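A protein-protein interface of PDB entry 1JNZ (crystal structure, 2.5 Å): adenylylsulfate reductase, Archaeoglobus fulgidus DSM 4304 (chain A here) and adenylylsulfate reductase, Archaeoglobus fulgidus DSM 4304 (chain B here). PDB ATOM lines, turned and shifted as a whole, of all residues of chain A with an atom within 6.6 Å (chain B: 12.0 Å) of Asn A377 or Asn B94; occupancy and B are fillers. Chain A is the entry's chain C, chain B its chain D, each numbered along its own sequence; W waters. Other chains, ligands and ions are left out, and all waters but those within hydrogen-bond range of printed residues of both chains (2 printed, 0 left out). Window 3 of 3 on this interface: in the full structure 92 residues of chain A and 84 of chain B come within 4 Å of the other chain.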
ATOM      1  N   LEU A 372      23.501   8.679  31.468  1.00  0.00           N
ATOM      2  CA  LEU A 372      24.764   8.610  30.741  1.00  0.00           C
ATOM      3  C   LEU A 372      24.564   9.259  29.376  1.00  0.00           C
ATOM      4  O   LEU A 372      25.386  10.066  28.928  1.00  0.00           O
ATOM      5  CB  LEU A 372      25.207   7.151  30.584  1.00  0.00           C
ATOM      6  CG  LEU A 372      26.540   6.867  29.868  1.00  0.00           C
ATOM      7  CD1 LEU A 372      26.956   5.433  30.118  1.00  0.00           C
ATOM      8  CD2 LEU A 372      26.401   7.127  28.367  1.00  0.00           C
ATOM      9  N   TRP A 373      23.460   8.913  28.720  1.00  0.00           N
ATOM     10  CA  TRP A 373      23.149   9.481  27.413  1.00  0.00           C
ATOM     11  C   TRP A 373      23.075  11.000  27.483  1.00  0.00           C
ATOM     12  O   TRP A 373      23.620  11.695  26.625  1.00  0.00           O
ATOM     13  CB  TRP A 373      21.811   8.944  26.890  1.00  0.00           C
ATOM     14  CG  TRP A 373      21.896   7.601  26.243  1.00  0.00           C
ATOM     15  CD1 TRP A 373      23.029   6.875  25.993  1.00  0.00           C
ATOM     16  CD2 TRP A 373      20.811   6.856  25.680  1.00  0.00           C
ATOM     17  NE1 TRP A 373      22.714   5.731  25.303  1.00  0.00           N
ATOM     18  CE2 TRP A 373      21.361   5.694  25.095  1.00  0.00           C
ATOM     19  CE3 TRP A 373      19.423   7.061  25.606  1.00  0.00           C
ATOM     20  CZ2 TRP A 373      20.572   4.738  24.442  1.00  0.00           C
ATOM     21  CZ3 TRP A 373      18.638   6.110  24.956  1.00  0.00           C
ATOM     22  CH2 TRP A 373      19.218   4.962  24.381  1.00  0.00           C
ATOM     23  N   ALA A 374      22.394  11.504  28.508  1.00  0.00           N
ATOM     24  CA  ALA A 374      22.230  12.940  28.695  1.00  0.00           C
ATOM     25  C   ALA A 374      23.554  13.646  28.977  1.00  0.00           C
ATOM     26  O   ALA A 374      23.844  14.682  28.385  1.00  0.00           O
ATOM     27  CB  ALA A 374      21.240  13.209  29.824  1.00  0.00           C
ATOM     28  N   CYS A 375      24.352  13.090  29.884  1.00  0.00           N
ATOM     29  CA  CYS A 375      25.640  13.689  30.221  1.00  0.00           C
ATOM     30  C   CYS A 375      26.612  13.678  29.035  1.00  0.00           C
ATOM     31  O   CYS A 375      27.436  14.581  28.891  1.00  0.00           O
ATOM     32  CB  CYS A 375      26.280  12.954  31.408  1.00  0.00           C
ATOM     33  SG  CYS A 375      25.436  13.152  33.005  1.00  0.00           S
ATOM     34  N   GLN A 376      26.510  12.661  28.186  1.00  0.00           N
ATOM     35  CA  GLN A 376      27.398  12.547  27.033  1.00  0.00           C
ATOM     36  C   GLN A 376      26.770  13.028  25.721  1.00  0.00           C
ATOM     37  O   GLN A 376      27.319  12.790  24.641  1.00  0.00           O
ATOM     38  CB  GLN A 376      27.884  11.092  26.892  1.00  0.00           C
ATOM     39  CG  GLN A 376      28.974  10.712  27.903  1.00  0.00           C
ATOM     40  CD  GLN A 376      29.378   9.239  27.867  1.00  0.00           C
ATOM     41  OE1 GLN A 376      29.379   8.600  26.820  1.00  0.00           O
ATOM     42  NE2 GLN A 376      29.751   8.707  29.023  1.00  0.00           N
ATOM     43  N   ASN A 377      25.633  13.714  25.822  1.00  0.00           N
ATOM     44  CA  ASN A 377      24.923  14.229  24.649  1.00  0.00           C
ATOM     45  C   ASN A 377      24.722  13.170  23.568  1.00  0.00           C
ATOM     46  O   ASN A 377      24.985  13.409  22.392  1.00  0.00           O
ATOM     47  CB  ASN A 377      25.660  15.431  24.040  1.00  0.00           C
ATOM     48  CG  ASN A 377      25.624  16.657  24.934  1.00  0.00           C
ATOM     49  OD1 ASN A 377      24.606  16.952  25.563  1.00  0.00           O
ATOM     50  ND2 ASN A 377      26.732  17.386  24.984  1.00  0.00           N
ATOM     51  N   ILE A 378      24.261  11.994  23.969  1.00  0.00           N
ATOM     52  CA  ILE A 378      24.020  10.931  23.011  1.00  0.00           C
ATOM     53  C   ILE A 378      22.520  10.830  22.755  1.00  0.00           C
ATOM     54  O   ILE A 378      21.739  10.599  23.678  1.00  0.00           O
ATOM     55  CB  ILE A 378      24.542   9.562  23.529  1.00  0.00           C
ATOM     56  CG1 ILE A 378      26.062   9.603  23.693  1.00  0.00           C
ATOM     57  CG2 ILE A 378      24.153   8.447  22.548  1.00  0.00           C
ATOM     58  CD1 ILE A 378      26.666   8.293  24.194  1.00  0.00           C
ATOM     59  N   ASP A 379      22.121  11.041  21.503  1.00  0.00           N
ATOM     60  CA  ASP A 379      20.719  10.952  21.117  1.00  0.00           C
ATOM     61  C   ASP A 379      20.563   9.683  20.289  1.00  0.00           C
ATOM     62  O   ASP A 379      20.913   9.654  19.109  1.00  0.00           O
ATOM     63  CB  ASP A 379      20.304  12.174  20.296  1.00  0.00           C
ATOM     64  CG  ASP A 379      18.850  12.112  19.850  1.00  0.00           C
ATOM     65  OD1 ASP A 379      18.378  13.084  19.223  1.00  0.00           O
ATOM     66  OD2 ASP A 379      18.180  11.089  20.123  1.00  0.00           O
ATOM     67  N   GLN A 383      23.032   8.883  17.039  1.00  0.00           N
ATOM     68  CA  GLN A 383      24.271   8.122  17.151  1.00  0.00           C
ATOM     69  C   GLN A 383      24.126   6.845  17.973  1.00  0.00           C
ATOM     70  O   GLN A 383      23.264   6.749  18.849  1.00  0.00           O
ATOM     71  CB  GLN A 383      25.404   8.991  17.723  1.00  0.00           C
ATOM     72  CG  GLN A 383      25.069   9.822  18.947  1.00  0.00           C
ATOM     73  CD  GLN A 383      24.365  11.128  18.605  1.00  0.00           C
ATOM     74  OE1 GLN A 383      24.701  11.789  17.622  1.00  0.00           O
ATOM     75  NE2 GLN A 383      23.397  11.514  19.428  1.00  0.00           N
ATOM     76  N   GLY B  66      25.351  12.026  37.939  1.00  0.00           N
ATOM     77  CA  GLY B  66      26.028  10.869  37.377  1.00  0.00           C
ATOM     78  C   GLY B  66      27.437  10.591  37.876  1.00  0.00           C
ATOM     79  O   GLY B  66      28.228  11.518  38.066  1.00  0.00           O
ATOM     80  N   TYR B  70      32.575   8.281  34.562  1.00  0.00           N
ATOM     81  CA  TYR B  70      32.270   8.368  33.140  1.00  0.00           C
ATOM     82  C   TYR B  70      31.275   9.446  32.741  1.00  0.00           C
ATOM     83  O   TYR B  70      30.990   9.620  31.551  1.00  0.00           O
ATOM     84  CB  TYR B  70      31.737   7.015  32.660  1.00  0.00           C
ATOM     85  CG  TYR B  70      30.438   6.584  33.328  1.00  0.00           C
ATOM     86  CD1 TYR B  70      29.214   7.164  32.975  1.00  0.00           C
ATOM     87  CD2 TYR B  70      30.428   5.571  34.291  1.00  0.00           C
ATOM     88  CE1 TYR B  70      28.015   6.740  33.559  1.00  0.00           C
ATOM     89  CE2 TYR B  70      29.234   5.141  34.880  1.00  0.00           C
ATOM     90  CZ  TYR B  70      28.033   5.725  34.507  1.00  0.00           C
ATOM     91  OH  TYR B  70      26.848   5.274  35.053  1.00  0.00           O
ATOM     92  N   SER B  71      30.752  10.169  33.724  1.00  0.00           N
ATOM     93  CA  SER B  71      29.751  11.192  33.454  1.00  0.00           C
ATOM     94  C   SER B  71      30.237  12.626  33.328  1.00  0.00           C
ATOM     95  O   SER B  71      30.790  13.192  34.271  1.00  0.00           O
ATOM     96  CB  SER B  71      28.668  11.159  34.535  1.00  0.00           C
ATOM     97  OG  SER B  71      28.094   9.875  34.647  1.00  0.00           O
ATOM     98  N   PRO B  72      30.059  13.230  32.143  1.00  0.00           N
ATOM     99  CA  PRO B  72      30.501  14.619  32.029  1.00  0.00           C
ATOM    100  C   PRO B  72      29.423  15.414  32.781  1.00  0.00           C
ATOM    101  O   PRO B  72      28.280  14.962  32.876  1.00  0.00           O
ATOM    102  CB  PRO B  72      30.465  14.868  30.521  1.00  0.00           C
ATOM    103  CG  PRO B  72      30.748  13.508  29.946  1.00  0.00           C
ATOM    104  CD  PRO B  72      29.881  12.630  30.808  1.00  0.00           C
ATOM    105  N   LEU B  73      29.770  16.571  33.329  1.00  0.00           N
ATOM    106  CA  LEU B  73      28.792  17.378  34.059  1.00  0.00           C
ATOM    107  C   LEU B  73      27.644  17.882  33.168  1.00  0.00           C
ATOM    108  O   LEU B  73      27.779  17.960  31.944  1.00  0.00           O
ATOM    109  CB  LEU B  73      29.486  18.585  34.702  1.00  0.00           C
ATOM    110  CG  LEU B  73      30.586  18.336  35.743  1.00  0.00           C
ATOM    111  CD1 LEU B  73      31.191  19.665  36.172  1.00  0.00           C
ATOM    112  CD2 LEU B  73      30.005  17.603  36.948  1.00  0.00           C
ATOM    113  N   GLY B  74      26.507  18.202  33.791  1.00  0.00           N
ATOM    114  CA  GLY B  74      25.384  18.741  33.044  1.00  0.00           C
ATOM    115  C   GLY B  74      24.144  17.898  32.805  1.00  0.00           C
ATOM    116  O   GLY B  74      23.060  18.448  32.612  1.00  0.00           O
ATOM    117  N   GLY B  75      24.280  16.577  32.812  1.00  0.00           N
ATOM    118  CA  GLY B  75      23.126  15.732  32.559  1.00  0.00           C
ATOM    119  C   GLY B  75      22.225  15.501  33.753  1.00  0.00           C
ATOM    120  O   GLY B  75      22.677  15.541  34.896  1.00  0.00           O
ATOM    121  N   ALA B  76      20.941  15.260  33.495  1.00  0.00           N
ATOM    122  CA  ALA B  76      20.003  15.003  34.583  1.00  0.00           C
ATOM    123  C   ALA B  76      18.711  14.341  34.128  1.00  0.00           C
ATOM    124  O   ALA B  76      18.240  14.552  33.010  1.00  0.00           O
ATOM    125  CB  ALA B  76      19.685  16.301  35.325  1.00  0.00           C
ATOM    126  N   CYS B  77      18.170  13.514  35.011  1.00  0.00           N
ATOM    127  CA  CYS B  77      16.911  12.826  34.784  1.00  0.00           C
ATOM    128  C   CYS B  77      16.102  13.154  36.023  1.00  0.00           C
ATOM    129  O   CYS B  77      16.502  12.816  37.134  1.00  0.00           O
ATOM    130  CB  CYS B  77      17.123  11.315  34.671  1.00  0.00           C
ATOM    131  SG  CYS B  77      17.964  10.829  33.157  1.00  0.00           S
ATOM    132  N   THR B  89      11.752  14.120  33.010  1.00  0.00           N
ATOM    133  CA  THR B  89      12.304  15.214  32.239  1.00  0.00           C
ATOM    134  C   THR B  89      13.762  14.812  32.130  1.00  0.00           C
ATOM    135  O   THR B  89      14.430  14.607  33.144  1.00  0.00           O
ATOM    136  CB  THR B  89      12.211  16.555  32.976  1.00  0.00           C
ATOM    137  OG1 THR B  89      10.836  16.902  33.157  1.00  0.00           O
ATOM    138  CG2 THR B  89      12.900  17.651  32.177  1.00  0.00           C
ATOM    139  N   VAL B  90      14.242  14.648  30.908  1.00  0.00           N
ATOM    140  CA  VAL B  90      15.627  14.279  30.711  1.00  0.00           C
ATOM    141  C   VAL B  90      16.312  15.504  30.148  1.00  0.00           C
ATOM    142  O   VAL B  90      15.943  16.000  29.076  1.00  0.00           O
ATOM    143  CB  VAL B  90      15.764  13.096  29.732  1.00  0.00           C
ATOM    144  CG1 VAL B  90      17.238  12.703  29.588  1.00  0.00           C
ATOM    145  CG2 VAL B  90      14.950  11.912  30.244  1.00  0.00           C
ATOM    146  N   LYS B  91      17.292  16.012  30.885  1.00  0.00           N
ATOM    147  CA  LYS B  91      18.000  17.197  30.442  1.00  0.00           C
ATOM    148  C   LYS B  91      19.435  16.867  30.059  1.00  0.00           C
ATOM    149  O   LYS B  91      20.211  16.359  30.870  1.00  0.00           O
ATOM    150  CB  LYS B  91      17.977  18.266  31.530  1.00  0.00           C
ATOM    151  CG  LYS B  91      18.535  19.603  31.045  1.00  0.00           C
ATOM    152  CD  LYS B  91      18.309  20.724  32.043  1.00  0.00           C
ATOM    153  CE  LYS B  91      18.584  22.082  31.402  1.00  0.00           C
ATOM    154  NZ  LYS B  91      18.199  23.226  32.291  1.00  0.00           N
ATOM    155  N   TYR B  92      19.774  17.180  28.812  1.00  0.00           N
ATOM    156  CA  TYR B  92      21.101  16.947  28.251  1.00  0.00           C
ATOM    157  C   TYR B  92      22.116  18.009  28.647  1.00  0.00           C
ATOM    158  O   TYR B  92      21.758  19.119  29.038  1.00  0.00           O
ATOM    159  CB  TYR B  92      21.018  16.895  26.719  1.00  0.00           C
ATOM    160  CG  TYR B  92      20.615  15.550  26.153  1.00  0.00           C
ATOM    161  CD1 TYR B  92      19.478  14.884  26.613  1.00  0.00           C
ATOM    162  CD2 TYR B  92      21.390  14.930  25.172  1.00  0.00           C
ATOM    163  CE1 TYR B  92      19.132  13.630  26.114  1.00  0.00           C
ATOM    164  CE2 TYR B  92      21.049  13.678  24.666  1.00  0.00           C
ATOM    165  CZ  TYR B  92      19.924  13.033  25.144  1.00  0.00           C
ATOM    166  OH  TYR B  92      19.613  11.773  24.681  1.00  0.00           O
ATOM    167  N   ARG B  93      23.391  17.654  28.537  1.00  0.00           N
ATOM    168  CA  ARG B  93      24.484  18.562  28.854  1.00  0.00           C
ATOM    169  C   ARG B  93      24.427  19.765  27.913  1.00  0.00           C
ATOM    170  O   ARG B  93      24.704  20.889  28.324  1.00  0.00           O
ATOM    171  CB  ARG B  93      25.818  17.823  28.700  1.00  0.00           C
ATOM    172  CG  ARG B  93      27.092  18.675  28.778  1.00  0.00           C
ATOM    173  CD  ARG B  93      28.302  17.772  28.519  1.00  0.00           C
ATOM    174  NE  ARG B  93      29.570  18.484  28.371  1.00  0.00           N
ATOM    175  CZ  ARG B  93      30.392  18.799  29.369  1.00  0.00           C
ATOM    176  NH1 ARG B  93      30.092  18.468  30.621  1.00  0.00           N
ATOM    177  NH2 ARG B  93      31.524  19.440  29.108  1.00  0.00           N
ATOM    178  N   ASN B  94      24.052  19.521  26.656  1.00  0.00           N
ATOM    179  CA  ASN B  94      23.966  20.579  25.654  1.00  0.00           C
ATOM    180  C   ASN B  94      22.706  21.445  25.743  1.00  0.00           C
ATOM    181  O   ASN B  94      22.523  22.353  24.931  1.00  0.00           O
ATOM    182  CB  ASN B  94      24.073  20.002  24.239  1.00  0.00           C
ATOM    183  CG  ASN B  94      22.936  19.059  23.898  1.00  0.00           C
ATOM    184  OD1 ASN B  94      21.821  19.207  24.392  1.00  0.00           O
ATOM    185  ND2 ASN B  94      23.212  18.089  23.031  1.00  0.00           N
ATOM    186  N   GLY B  95      21.838  21.155  26.713  1.00  0.00           N
ATOM    187  CA  GLY B  95      20.629  21.946  26.888  1.00  0.00           C
ATOM    188  C   GLY B  95      19.322  21.352  26.390  1.00  0.00           C
ATOM    189  O   GLY B  95      18.247  21.907  26.640  1.00  0.00           O
ATOM    190  N   LYS B  96      19.402  20.230  25.684  1.00  0.00           N
ATOM    191  CA  LYS B  96      18.224  19.561  25.152  1.00  0.00           C
ATOM    192  C   LYS B  96      17.377  19.040  26.304  1.00  0.00           C
ATOM    193  O   LYS B  96      17.908  18.602  27.324  1.00  0.00           O
ATOM    194  CB  LYS B  96      18.640  18.395  24.261  1.00  0.00           C
ATOM    195  CG  LYS B  96      17.483  17.645  23.640  1.00  0.00           C
ATOM    196  CD  LYS B  96      17.993  16.531  22.745  1.00  0.00           C
ATOM    197  CE  LYS B  96      16.868  15.911  21.945  1.00  0.00           C
ATOM    198  NZ  LYS B  96      17.391  14.926  20.966  1.00  0.00           N
ATOM    199  N   VAL B  97      16.061  19.149  26.155  1.00  0.00           N
ATOM    200  CA  VAL B  97      15.141  18.704  27.188  1.00  0.00           C
ATOM    201  C   VAL B  97      14.065  17.816  26.602  1.00  0.00           C
ATOM    202  O   VAL B  97      13.341  18.212  25.690  1.00  0.00           O
ATOM    203  CB  VAL B  97      14.473  19.905  27.906  1.00  0.00           C
ATOM    204  CG1 VAL B  97      13.430  19.411  28.905  1.00  0.00           C
ATOM    205  CG2 VAL B  97      15.525  20.721  28.631  1.00  0.00           C
ATOM    206  N   LEU B  98      13.981  16.601  27.130  1.00  0.00           N
ATOM    207  CA  LEU B  98      12.990  15.634  26.692  1.00  0.00           C
ATOM    208  C   LEU B  98      12.008  15.451  27.838  1.00  0.00           C
ATOM    209  O   LEU B  98      12.368  15.615  29.005  1.00  0.00           O
ATOM    210  CB  LEU B  98      13.664  14.302  26.374  1.00  0.00           C
ATOM    211  CG  LEU B  98      14.784  14.382  25.337  1.00  0.00           C
ATOM    212  CD1 LEU B  98      15.542  13.061  25.300  1.00  0.00           C
ATOM    213  CD2 LEU B  98      14.193  14.718  23.970  1.00  0.00           C
HETATM  214  O   HOH W   1      24.498  13.943  36.035  1.00  0.00           O
HETATM  215  O   HOH W   2      25.638   9.485  33.595  1.00  0.00           O
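The backbone NH (N) of Arg B93 lies within hydrogen-bond range of the backbone carbonyl oxygen (O) of Ala A374, 3.0 Å away.
The backbone carbonyl oxygen (O) of Pro B72 lies close to the side-chain sulfur (SG) of Cys A375, 3.4 Å away.
N of Gly B75 sits close to SG of Cys A375 (3.6 Å).
The side-chain amide nitrogen of Gln A376 sits at hydrogen-bond distance from the backbone carbonyl oxygen of Tyr B70.
N of Arg B93 lies within hydrogen-bond range of OD1 of Asn A377, at 3.3 Å.
OD1 of Asn A377 is in hydrogen-bond range of N of Asn B94 (2.8 Å).
The side-chain hydroxyl of Tyr B92 sits at hydrogen-bond distance from the backbone carbonyl oxygen of Ile A378.
OD1 of Asp A379 is in salt-bridge range of NZ of Lys B96, 2.7 Å away.
Among the printed residues, merely in contact across the chains: Leu A372 with Tyr B70 (3.8 Å), Trp A373 with Tyr B92 (3.8 Å), Ala A374 with Lys B91 (3.5 Å), Ala A374 with Tyr B92 (3.6 Å), Cys A375 with Arg B93 (3.3 Å), Gln A376 with Pro B72 (3.6 Å), Asn A377 with Tyr B92 (3.6 Å) and Asp A379 with Tyr B92 (3.8 Å).
O of Trp A373 is in hydrogen-bond range of N of Ile A378.
The side-chain amide nitrogen of Gln A383 lies close to the backbone NH of Asp A379, at 2.5 Å.
NH1 of Arg B93 is in hydrogen-bond range of O of Leu B73, at 2.7 Å.
N of Lys B91 sits at hydrogen-bond distance from O of Ala B76.
The backbone NH (N) of Lys B96 is in hydrogen-bond range of the side-chain amide oxygen (OD1) of Asn B94 (2.9 Å).
Water W1 lies within hydrogen-bond range of O of Gly B75 (2.7 Å), N of Gly B66 (2.8 Å) and SG of Cys A375 (3.3 Å).
Water W2 lies within hydrogen-bond range of the side-chain hydroxyl (OG) of Ser B71 (2.7 Å), the backbone NH (N) of Leu A372 (3.1 Å) and the side-chain sulfur (SG) of Cys A375 (3.7 Å).
Hydrophobic or aromatic side chains of chain B within 4 Å of the printed part of chain A: Tyr B70, Pro B72 and Tyr B92.
Of the 9 printed residues of chain A, 8 touch a printed residue of chain B.
Along chain A the printed residues that touch a printed residue of chain B span positions 372 to 379.
Among the printed residues, 16 pairs touch across the chains.
Among the printed residues, Asp or Glu carboxylates within 4 Å of a Lys or Arg side-chain nitrogen of the other chain: Asp A379 with Lys B96 (2.7 Å).
Asn A377 touches just these residues of chain B: Tyr B92, Arg B93 and Asn B94.
Of chain A, only Asn A377 comes within 4 Å of Asn B94.
Of chain B, only Lys B91, Tyr B92 and Arg B93 come within 4 Å of Ala A374.
Gln A376 touches two residues of chain B.
Ile A378 touches one residue of chain B.
Of the printed residues of chain A, Arg B93 touches Ala A374, Cys A375 and Asn A377.
Of the printed residues of chain A, Lys B91 touches Ala A374.
Printed residues of chain B within 4 Å of Trp A373: Tyr B92.
Val B90 touches none of the printed residues of chain A.
The nearest residue of chain B that does not touch Asn A377 is Gly B95 (5.2 Å).
The nearest printed residue of chain A that does not touch Lys B91 is Cys A375 (5.4 Å).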
